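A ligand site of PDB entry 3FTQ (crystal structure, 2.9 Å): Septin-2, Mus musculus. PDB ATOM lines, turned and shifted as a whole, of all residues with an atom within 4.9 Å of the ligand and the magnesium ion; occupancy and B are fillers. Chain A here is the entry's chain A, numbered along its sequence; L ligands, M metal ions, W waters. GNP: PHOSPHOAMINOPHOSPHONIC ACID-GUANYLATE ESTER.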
ATOM      1  N   GLU A  13      16.839   0.778  -3.760  1.00  0.00           N
ATOM      2  CA  GLU A  13      17.523  -0.091  -2.822  1.00  0.00           C
ATOM      3  C   GLU A  13      16.610  -0.525  -1.668  1.00  0.00           C
ATOM      4  O   GLU A  13      15.750   0.235  -1.236  1.00  0.00           O
ATOM      5  CB  GLU A  13      18.772   0.633  -2.285  1.00  0.00           C
ATOM      6  CG  GLU A  13      19.468  -0.001  -1.086  1.00  0.00           C
ATOM      7  CD  GLU A  13      20.896   0.477  -0.923  1.00  0.00           C
ATOM      8  OE1 GLU A  13      21.145   1.698  -1.037  1.00  0.00           O
ATOM      9  OE2 GLU A  13      21.783  -0.392  -0.686  1.00  0.00           O
ATOM     10  N   SER A  14      16.811  -1.751  -1.200  1.00  0.00           N
ATOM     11  CA  SER A  14      16.038  -2.308  -0.098  1.00  0.00           C
ATOM     12  C   SER A  14      16.255  -1.498   1.177  1.00  0.00           C
ATOM     13  O   SER A  14      17.324  -0.920   1.384  1.00  0.00           O
ATOM     14  CB  SER A  14      16.447  -3.759   0.130  1.00  0.00           C
ATOM     15  OG  SER A  14      15.666  -4.337   1.167  1.00  0.00           O
ATOM     16  N   GLY A  15      15.226  -1.443   2.027  1.00  0.00           N
ATOM     17  CA  GLY A  15      15.289  -0.722   3.306  1.00  0.00           C
ATOM     18  C   GLY A  15      15.316   0.786   3.221  1.00  0.00           C
ATOM     19  O   GLY A  15      15.795   1.456   4.139  1.00  0.00           O
ATOM     20  N   LEU A  16      14.816   1.347   2.119  1.00  0.00           N
ATOM     21  CA  LEU A  16      14.748   2.793   1.976  1.00  0.00           C
ATOM     22  C   LEU A  16      13.360   3.376   2.275  1.00  0.00           C
ATOM     23  O   LEU A  16      13.102   4.555   2.025  1.00  0.00           O
ATOM     24  CB  LEU A  16      15.211   3.222   0.588  1.00  0.00           C
ATOM     25  CG  LEU A  16      16.697   3.073   0.259  1.00  0.00           C
ATOM     26  CD1 LEU A  16      16.969   3.643  -1.111  1.00  0.00           C
ATOM     27  CD2 LEU A  16      17.596   3.756   1.319  1.00  0.00           C
ATOM     28  N   GLY A  17      12.467   2.555   2.832  1.00  0.00           N
ATOM     29  CA  GLY A  17      11.157   3.027   3.255  1.00  0.00           C
ATOM     30  C   GLY A  17      10.149   3.139   2.126  1.00  0.00           C
ATOM     31  O   GLY A  17       9.189   3.902   2.203  1.00  0.00           O
ATOM     32  N   LYS A  18      10.360   2.362   1.071  1.00  0.00           N
ATOM     33  CA  LYS A  18       9.517   2.417  -0.130  1.00  0.00           C
ATOM     34  C   LYS A  18       8.072   2.010   0.176  1.00  0.00           C
ATOM     35  O   LYS A  18       7.154   2.771  -0.086  1.00  0.00           O
ATOM     36  CB  LYS A  18      10.069   1.511  -1.217  1.00  0.00           C
ATOM     37  CG  LYS A  18      11.380   1.966  -1.798  1.00  0.00           C
ATOM     38  CD  LYS A  18      11.734   1.170  -3.058  1.00  0.00           C
ATOM     39  CE  LYS A  18      11.984  -0.309  -2.774  1.00  0.00           C
ATOM     40  NZ  LYS A  18      13.234  -0.550  -1.988  1.00  0.00           N
ATOM     41  N   SER A  19       7.890   0.816   0.750  1.00  0.00           N
ATOM     42  CA  SER A  19       6.561   0.331   1.097  1.00  0.00           C
ATOM     43  C   SER A  19       5.887   1.267   2.092  1.00  0.00           C
ATOM     44  O   SER A  19       4.697   1.493   1.985  1.00  0.00           O
ATOM     45  CB  SER A  19       6.615  -1.072   1.680  1.00  0.00           C
ATOM     46  OG  SER A  19       7.304  -1.946   0.807  1.00  0.00           O
ATOM     47  N   THR A  20       6.656   1.816   3.035  1.00  0.00           N
ATOM     48  CA  THR A  20       6.087   2.681   4.049  1.00  0.00           C
ATOM     49  C   THR A  20       5.514   3.926   3.398  1.00  0.00           C
ATOM     50  O   THR A  20       4.427   4.373   3.764  1.00  0.00           O
ATOM     51  CB  THR A  20       7.127   3.089   5.144  1.00  0.00           C
ATOM     52  OG1 THR A  20       7.674   1.914   5.768  1.00  0.00           O
ATOM     53  CG2 THR A  20       6.487   3.955   6.222  1.00  0.00           C
ATOM     54  N   ILE A  43       3.437  -4.383   8.256  1.00  0.00           N
ATOM     55  CA  ILE A  43       4.298  -3.933   7.165  1.00  0.00           C
ATOM     56  C   ILE A  43       5.639  -4.552   6.787  1.00  0.00           C
ATOM     57  O   ILE A  43       6.660  -3.850   6.723  1.00  0.00           O
ATOM     58  CB  ILE A  43       4.586  -2.420   7.342  1.00  0.00           C
ATOM     59  CG1 ILE A  43       4.902  -1.783   5.995  1.00  0.00           C
ATOM     60  CG2 ILE A  43       5.730  -2.205   8.325  1.00  0.00           C
ATOM     61  CD1 ILE A  43       6.129  -0.890   6.014  1.00  0.00           C
ATOM     62  N   GLU A  44       5.637  -5.850   6.524  1.00  0.00           N
ATOM     63  CA  GLU A  44       6.853  -6.541   6.067  1.00  0.00           C
ATOM     64  C   GLU A  44       7.686  -6.237   4.824  1.00  0.00           C
ATOM     65  O   GLU A  44       7.245  -5.542   3.902  1.00  0.00           O
ATOM     66  CB  GLU A  44       6.453  -8.016   5.997  1.00  0.00           C
ATOM     67  CG  GLU A  44       5.623  -8.495   7.185  1.00  0.00           C
ATOM     68  CD  GLU A  44       4.612  -9.574   6.808  1.00  0.00           C
ATOM     69  OE1 GLU A  44       4.144  -9.584   5.640  1.00  0.00           O
ATOM     70  OE2 GLU A  44       4.281 -10.411   7.682  1.00  0.00           O
ATOM     71  N   ARG A  45       8.890  -6.778   4.816  1.00  0.00           N
ATOM     72  CA  ARG A  45       9.772  -6.736   3.672  1.00  0.00           C
ATOM     73  C   ARG A  45       9.069  -7.214   2.391  1.00  0.00           C
ATOM     74  O   ARG A  45       8.457  -8.282   2.389  1.00  0.00           O
ATOM     75  CB  ARG A  45      10.999  -7.589   3.959  1.00  0.00           C
ATOM     76  CG  ARG A  45      11.690  -8.077   2.722  1.00  0.00           C
ATOM     77  CD  ARG A  45      12.793  -9.025   3.049  1.00  0.00           C
ATOM     78  NE  ARG A  45      13.954  -8.695   2.231  1.00  0.00           N
ATOM     79  CZ  ARG A  45      15.194  -9.064   2.519  1.00  0.00           C
ATOM     80  NH1 ARG A  45      15.435  -9.779   3.623  1.00  0.00           N
ATOM     81  NH2 ARG A  45      16.182  -8.698   1.723  1.00  0.00           N
ATOM     82  N   THR A  46       9.163  -6.425   1.324  1.00  0.00           N
ATOM     83  CA  THR A  46       8.519  -6.750   0.056  1.00  0.00           C
ATOM     84  C   THR A  46       9.331  -7.788  -0.709  1.00  0.00           C
ATOM     85  O   THR A  46      10.477  -7.550  -1.055  1.00  0.00           O
ATOM     86  CB  THR A  46       8.367  -5.495  -0.821  1.00  0.00           C
ATOM     87  OG1 THR A  46       7.951  -4.386   0.002  1.00  0.00           O
ATOM     88  CG2 THR A  46       7.333  -5.719  -1.910  1.00  0.00           C
ATOM     89  N   ASP A  69       4.466  -1.844  -5.841  1.00  0.00           N
ATOM     90  CA  ASP A  69       5.576  -1.978  -4.932  1.00  0.00           C
ATOM     91  C   ASP A  69       6.530  -3.047  -5.464  1.00  0.00           C
ATOM     92  O   ASP A  69       6.108  -4.078  -5.996  1.00  0.00           O
ATOM     93  CB  ASP A  69       5.071  -2.374  -3.550  1.00  0.00           C
ATOM     94  CG  ASP A  69       6.056  -2.033  -2.436  1.00  0.00           C
ATOM     95  OD1 ASP A  69       7.224  -1.696  -2.723  1.00  0.00           O
ATOM     96  OD2 ASP A  69       5.637  -2.112  -1.264  1.00  0.00           O
ATOM     97  N   THR A  70       7.824  -2.783  -5.343  1.00  0.00           N
ATOM     98  CA  THR A  70       8.836  -3.694  -5.828  1.00  0.00           C
ATOM     99  C   THR A  70       9.802  -4.044  -4.699  1.00  0.00           C
ATOM    100  O   THR A  70      10.019  -3.215  -3.812  1.00  0.00           O
ATOM    101  CB  THR A  70       9.607  -3.099  -7.006  1.00  0.00           C
ATOM    102  OG1 THR A  70      10.373  -1.969  -6.557  1.00  0.00           O
ATOM    103  CG2 THR A  70       8.642  -2.637  -8.104  1.00  0.00           C
ATOM    104  N   PRO A  71      10.346  -5.279  -4.705  1.00  0.00           N
ATOM    105  CA  PRO A  71      11.441  -5.599  -3.801  1.00  0.00           C
ATOM    106  C   PRO A  71      12.718  -4.833  -4.154  1.00  0.00           C
ATOM    107  O   PRO A  71      13.110  -4.814  -5.313  1.00  0.00           O
ATOM    108  CB  PRO A  71      11.635  -7.111  -3.999  1.00  0.00           C
ATOM    109  CG  PRO A  71      10.970  -7.437  -5.268  1.00  0.00           C
ATOM    110  CD  PRO A  71       9.913  -6.438  -5.516  1.00  0.00           C
ATOM    111  N   GLY A  72      13.330  -4.199  -3.152  1.00  0.00           N
ATOM    112  CA  GLY A  72      14.577  -3.447  -3.329  1.00  0.00           C
ATOM    113  C   GLY A  72      15.798  -4.338  -3.445  1.00  0.00           C
ATOM    114  O   GLY A  72      15.764  -5.502  -3.011  1.00  0.00           O
ATOM    115  N   LYS A 151      14.064   8.399   3.344  1.00  0.00           N
ATOM    116  CA  LYS A 151      14.327   8.585   4.771  1.00  0.00           C
ATOM    117  C   LYS A 151      15.050   9.893   5.077  1.00  0.00           C
ATOM    118  O   LYS A 151      16.110   9.913   5.687  1.00  0.00           O
ATOM    119  CB  LYS A 151      15.109   7.366   5.303  1.00  0.00           C
ATOM    120  CG  LYS A 151      14.356   6.044   5.145  1.00  0.00           C
ATOM    121  CD  LYS A 151      15.009   4.936   5.921  1.00  0.00           C
ATOM    122  CE  LYS A 151      14.254   3.642   5.763  1.00  0.00           C
ATOM    123  NZ  LYS A 151      14.857   2.517   6.524  1.00  0.00           N
ATOM    124  N   ASP A 153      14.575  12.154   7.136  1.00  0.00           N
ATOM    125  CA  ASP A 153      14.757  12.483   8.546  1.00  0.00           C
ATOM    126  C   ASP A 153      16.149  12.090   9.073  1.00  0.00           C
ATOM    127  O   ASP A 153      16.471  12.301  10.246  1.00  0.00           O
ATOM    128  CB  ASP A 153      13.647  11.886   9.413  1.00  0.00           C
ATOM    129  CG  ASP A 153      13.478  10.389   9.201  1.00  0.00           C
ATOM    130  OD1 ASP A 153      13.974   9.837   8.202  1.00  0.00           O
ATOM    131  OD2 ASP A 153      12.821   9.763  10.046  1.00  0.00           O
ATOM    132  N   THR A 154      16.958  11.501   8.201  1.00  0.00           N
ATOM    133  CA  THR A 154      18.345  11.171   8.517  1.00  0.00           C
ATOM    134  C   THR A 154      19.244  12.309   8.048  1.00  0.00           C
ATOM    135  O   THR A 154      20.459  12.287   8.253  1.00  0.00           O
ATOM    136  CB  THR A 154      18.778   9.832   7.857  1.00  0.00           C
ATOM    137  OG1 THR A 154      19.186  10.056   6.506  1.00  0.00           O
ATOM    138  CG2 THR A 154      17.619   8.844   7.850  1.00  0.00           C
ATOM    139  N   VAL A 207      11.924  12.798   1.161  1.00  0.00           N
ATOM    140  CA  VAL A 207      10.691  12.375   1.800  1.00  0.00           C
ATOM    141  C   VAL A 207      10.881  11.538   3.071  1.00  0.00           C
ATOM    142  O   VAL A 207      11.937  10.958   3.295  1.00  0.00           O
ATOM    143  CB  VAL A 207       9.768  11.610   0.830  1.00  0.00           C
ATOM    144  CG1 VAL A 207       9.301  12.522  -0.298  1.00  0.00           C
ATOM    145  CG2 VAL A 207      10.464  10.365   0.279  1.00  0.00           C
ATOM    146  N   VAL A 208       9.827  11.521   3.890  1.00  0.00           N
ATOM    147  CA  VAL A 208       9.754  10.715   5.098  1.00  0.00           C
ATOM    148  C   VAL A 208       8.404   9.997   5.070  1.00  0.00           C
ATOM    149  O   VAL A 208       7.377  10.603   4.769  1.00  0.00           O
ATOM    150  CB  VAL A 208       9.845  11.601   6.361  1.00  0.00           C
ATOM    151  CG1 VAL A 208       9.694  10.760   7.625  1.00  0.00           C
ATOM    152  CG2 VAL A 208      11.152  12.351   6.397  1.00  0.00           C
ATOM    153  N   GLY A 209       8.400   8.704   5.381  1.00  0.00           N
ATOM    154  CA  GLY A 209       7.163   7.943   5.443  1.00  0.00           C
ATOM    155  C   GLY A 209       6.922   7.368   6.821  1.00  0.00           C
ATOM    156  O   GLY A 209       7.874   7.079   7.549  1.00  0.00           O
ATOM    157  N   ARG A 224       6.746  10.164  13.365  1.00  0.00           N
ATOM    158  CA  ARG A 224       8.052   9.579  13.696  1.00  0.00           C
ATOM    159  C   ARG A 224       8.481  10.104  15.062  1.00  0.00           C
ATOM    160  O   ARG A 224       8.916  11.254  15.208  1.00  0.00           O
ATOM    161  CB  ARG A 224       9.167   9.734  12.668  1.00  0.00           C
ATOM    162  CG  ARG A 224       9.138   8.684  11.591  1.00  0.00           C
ATOM    163  CD  ARG A 224      10.516   8.377  11.045  1.00  0.00           C
ATOM    164  NE  ARG A 224      10.644   6.945  10.835  1.00  0.00           N
ATOM    165  CZ  ARG A 224      11.465   6.137  11.492  1.00  0.00           C
ATOM    166  NH1 ARG A 224      12.311   6.593  12.404  1.00  0.00           N
ATOM    167  NH2 ARG A 224      11.452   4.846  11.222  1.00  0.00           N
ATOM    168  N   TYR A 226      10.908  10.270  17.918  1.00  0.00           N
ATOM    169  CA  TYR A 226      12.248  10.162  18.503  1.00  0.00           C
ATOM    170  C   TYR A 226      12.283  10.857  19.874  1.00  0.00           C
ATOM    171  O   TYR A 226      11.512  11.778  20.119  1.00  0.00           O
ATOM    172  CB  TYR A 226      13.282  10.854  17.596  1.00  0.00           C
ATOM    173  CG  TYR A 226      13.450  10.260  16.214  1.00  0.00           C
ATOM    174  CD1 TYR A 226      13.870   8.942  16.043  1.00  0.00           C
ATOM    175  CD2 TYR A 226      13.225  11.027  15.076  1.00  0.00           C
ATOM    176  CE1 TYR A 226      14.045   8.395  14.768  1.00  0.00           C
ATOM    177  CE2 TYR A 226      13.389  10.493  13.816  1.00  0.00           C
ATOM    178  CZ  TYR A 226      13.798   9.181  13.666  1.00  0.00           C
ATOM    179  OH  TYR A 226      13.961   8.661  12.406  1.00  0.00           O
HETATM  180  PG  GNP L   1      12.092  -3.474   0.808  1.00  0.00           P
HETATM  181  O1G GNP L   1      10.739  -4.151   0.838  1.00  0.00           O
HETATM  182  O2G GNP L   1      12.522  -2.872  -0.512  1.00  0.00           O
HETATM  183  O3G GNP L   1      13.041  -4.510   1.345  1.00  0.00           O
HETATM  184  N3B GNP L   1      12.072  -2.307   1.895  1.00  0.00           N
HETATM  185  PB  GNP L   1      11.345  -0.896   1.750  1.00  0.00           P
HETATM  186  O1B GNP L   1      12.143  -0.003   0.856  1.00  0.00           O
HETATM  187  O2B GNP L   1       9.952  -1.166   1.325  1.00  0.00           O
HETATM  188  O3A GNP L   1      11.324  -0.264   3.162  1.00  0.00           O
HETATM  189  PA  GNP L   1      10.145  -0.352   4.163  1.00  0.00           P
HETATM  190  O1A GNP L   1       9.084   0.574   3.722  1.00  0.00           O
HETATM  191  O2A GNP L   1       9.778  -1.756   4.428  1.00  0.00           O
HETATM  192  O5' GNP L   1      10.650   0.222   5.531  1.00  0.00           O
HETATM  193  C5' GNP L   1      11.744  -0.355   6.251  1.00  0.00           C
HETATM  194  C4' GNP L   1      11.783   0.290   7.613  1.00  0.00           C
HETATM  195  O4' GNP L   1      12.272   1.657   7.503  1.00  0.00           O
HETATM  196  C3' GNP L   1      10.384   0.467   8.183  1.00  0.00           C
HETATM  197  O3' GNP L   1      10.080  -0.717   8.878  1.00  0.00           O
HETATM  198  C2' GNP L   1      10.502   1.670   9.109  1.00  0.00           C
HETATM  199  O2' GNP L   1      10.801   1.244  10.427  1.00  0.00           O
HETATM  200  C1' GNP L   1      11.690   2.435   8.530  1.00  0.00           C
HETATM  201  N9  GNP L   1      11.306   3.694   7.921  1.00  0.00           N
HETATM  202  C8  GNP L   1      10.243   3.858   7.055  1.00  0.00           C
HETATM  203  N7  GNP L   1      10.092   5.079   6.623  1.00  0.00           N
HETATM  204  C5  GNP L   1      11.123   5.756   7.244  1.00  0.00           C
HETATM  205  C6  GNP L   1      11.454   7.103   7.140  1.00  0.00           C
HETATM  206  O6  GNP L   1      10.870   7.958   6.471  1.00  0.00           O
HETATM  207  N1  GNP L   1      12.560   7.434   7.900  1.00  0.00           N
HETATM  208  C2  GNP L   1      13.266   6.558   8.668  1.00  0.00           C
HETATM  209  N2  GNP L   1      14.306   7.100   9.306  1.00  0.00           N
HETATM  210  N3  GNP L   1      12.981   5.263   8.780  1.00  0.00           N
HETATM  211  C4  GNP L   1      11.885   4.925   8.041  1.00  0.00           C
HETATM  212 MG    MG M   1       9.327  -2.841   0.697  1.00  0.00          MG
HETATM  213  O   HOH W   1      12.817  -6.843   0.211  1.00  0.00           O
HETATM  214  O   HOH W   2       9.444  -2.201  -1.053  1.00  0.00           O
HETATM  215  O   HOH W   3       8.667  -3.336   2.642  1.00  0.00           O
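Along chain A the residues within 4 Å of the magnesium ion span positions 19 to 46.
The backbone NH (N) of Gly 15 lies close to a nitrogen (N3B) of the ligand (3.3 Å). Merely in contact with the ligand: Val 208 and Arg 45. Within 4 Å of the ligand: Ser 14, Gly 15, Leu 16, Gly 17, Lys 18, Ser 19, Thr 20, Arg 45, Thr 46, Gly 72, Lys 151, Asp 153, Val 208, Gly 209, Arg 224 and Tyr 226. The nearest printed residue that does not touch the ligand is Ile 43 (4.02 Å).
Water W2 is bound to the magnesium ion, at 1.9 Å. The magnesium ion is bound by an oxygen (O2B) of the ligand (1.9 Å). O1G of the ligand is bound to the magnesium ion (1.9 Å). Water W3 is bound to the magnesium ion. The magnesium ion is bound by OG1 of Thr 46, at 2.2 Å. OG of Ser 19 is bound to the magnesium ion, 2.2 Å away. The magnesium ion has six donor atoms within binding distance.
OD2 of Asp 69 sits close to OG of Ser 19, at 2.7 Å. The side-chain carboxylate (OD2) of Asp 153 lies within salt-bridge range of the guanidinium group (NE) of Arg 224 (3.6 Å). The side-chain carboxylate (OD2) of Asp 153 sits at hydrogen-bond distance from the side-chain hydroxyl (OH) of Tyr 226. The side-chain amino group (NZ) of Lys 18 lies within hydrogen-bond range of the backbone carbonyl oxygen (O) of Glu 13 (2.7 Å). NZ of Lys 151 lies within hydrogen-bond range of O of Gly 15 (2.8 Å). O of Lys 151 sits close to OG1 of Thr 154, 3.2 Å away. The backbone carbonyl oxygen (O) of Val 207 lies within hydrogen-bond range of the backbone NH (N) of Lys 151. NH1 of Arg 224 sits at hydrogen-bond distance from OH of Tyr 226 (2.6 Å).
Water W3 lies within hydrogen-bond range of O2A of the ligand (2.6 Å), O of Glu 44 (2.9 Å) and N of Thr 46 (3.4 Å). Water W2 lies within hydrogen-bond range of OD1 of Asp 69, O of Thr 70 and O2G of the ligand. Water W1 lies within hydrogen-bond range of an oxygen (O3G) of the ligand, the backbone carbonyl oxygen (O) of Thr 46 and the guanidinium group (NE) of Arg 45.
N of Thr 46 sits close to O1G of the ligand, 2.8 Å away. O1A of the ligand lies within hydrogen-bond range of N of Ser 19 (3.2 Å). OG of Ser 14 is in hydrogen-bond range of O3G of the ligand, 2.6 Å away. N of Gly 209 is in hydrogen-bond range of O6 of the ligand (2.8 Å). The backbone carbonyl oxygen of Gly 209 lies close to a nitrogen (N7) of the ligand, 3.1 Å away. OD1 of Asp 153 is in hydrogen-bond range of N1 of the ligand. O1A of the ligand lies within hydrogen-bond range of N of Thr 20, at 2.8 Å. The side-chain hydroxyl (OG1) of Thr 20 lies within hydrogen-bond range of an oxygen (O1A) of the ligand. An oxygen (O1B) of the ligand is in hydrogen-bond range of the backbone NH of Lys 18 (3.0 Å). An oxygen (O2G) of the ligand is in salt-bridge range of the side-chain amino group (NZ) of Lys 18, at 2.8 Å. The side-chain amino group of Lys 151 is in hydrogen-bond range of an oxygen (O4') of the ligand, at 2.9 Å. N3 of the ligand sits at hydrogen-bond distance from NH2 of Arg 224, at 2.9 Å. N of Gly 17 is in hydrogen-bond range of O3A of the ligand (3.1 Å). The backbone NH of Gly 72 is in hydrogen-bond range of an oxygen (O2G) of the ligand (3.1 Å). O1B of the ligand sits at hydrogen-bond distance from N of Leu 16 (3.3 Å). OH of Tyr 226 is in hydrogen-bond range of N2 of the ligand (3.5 Å).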
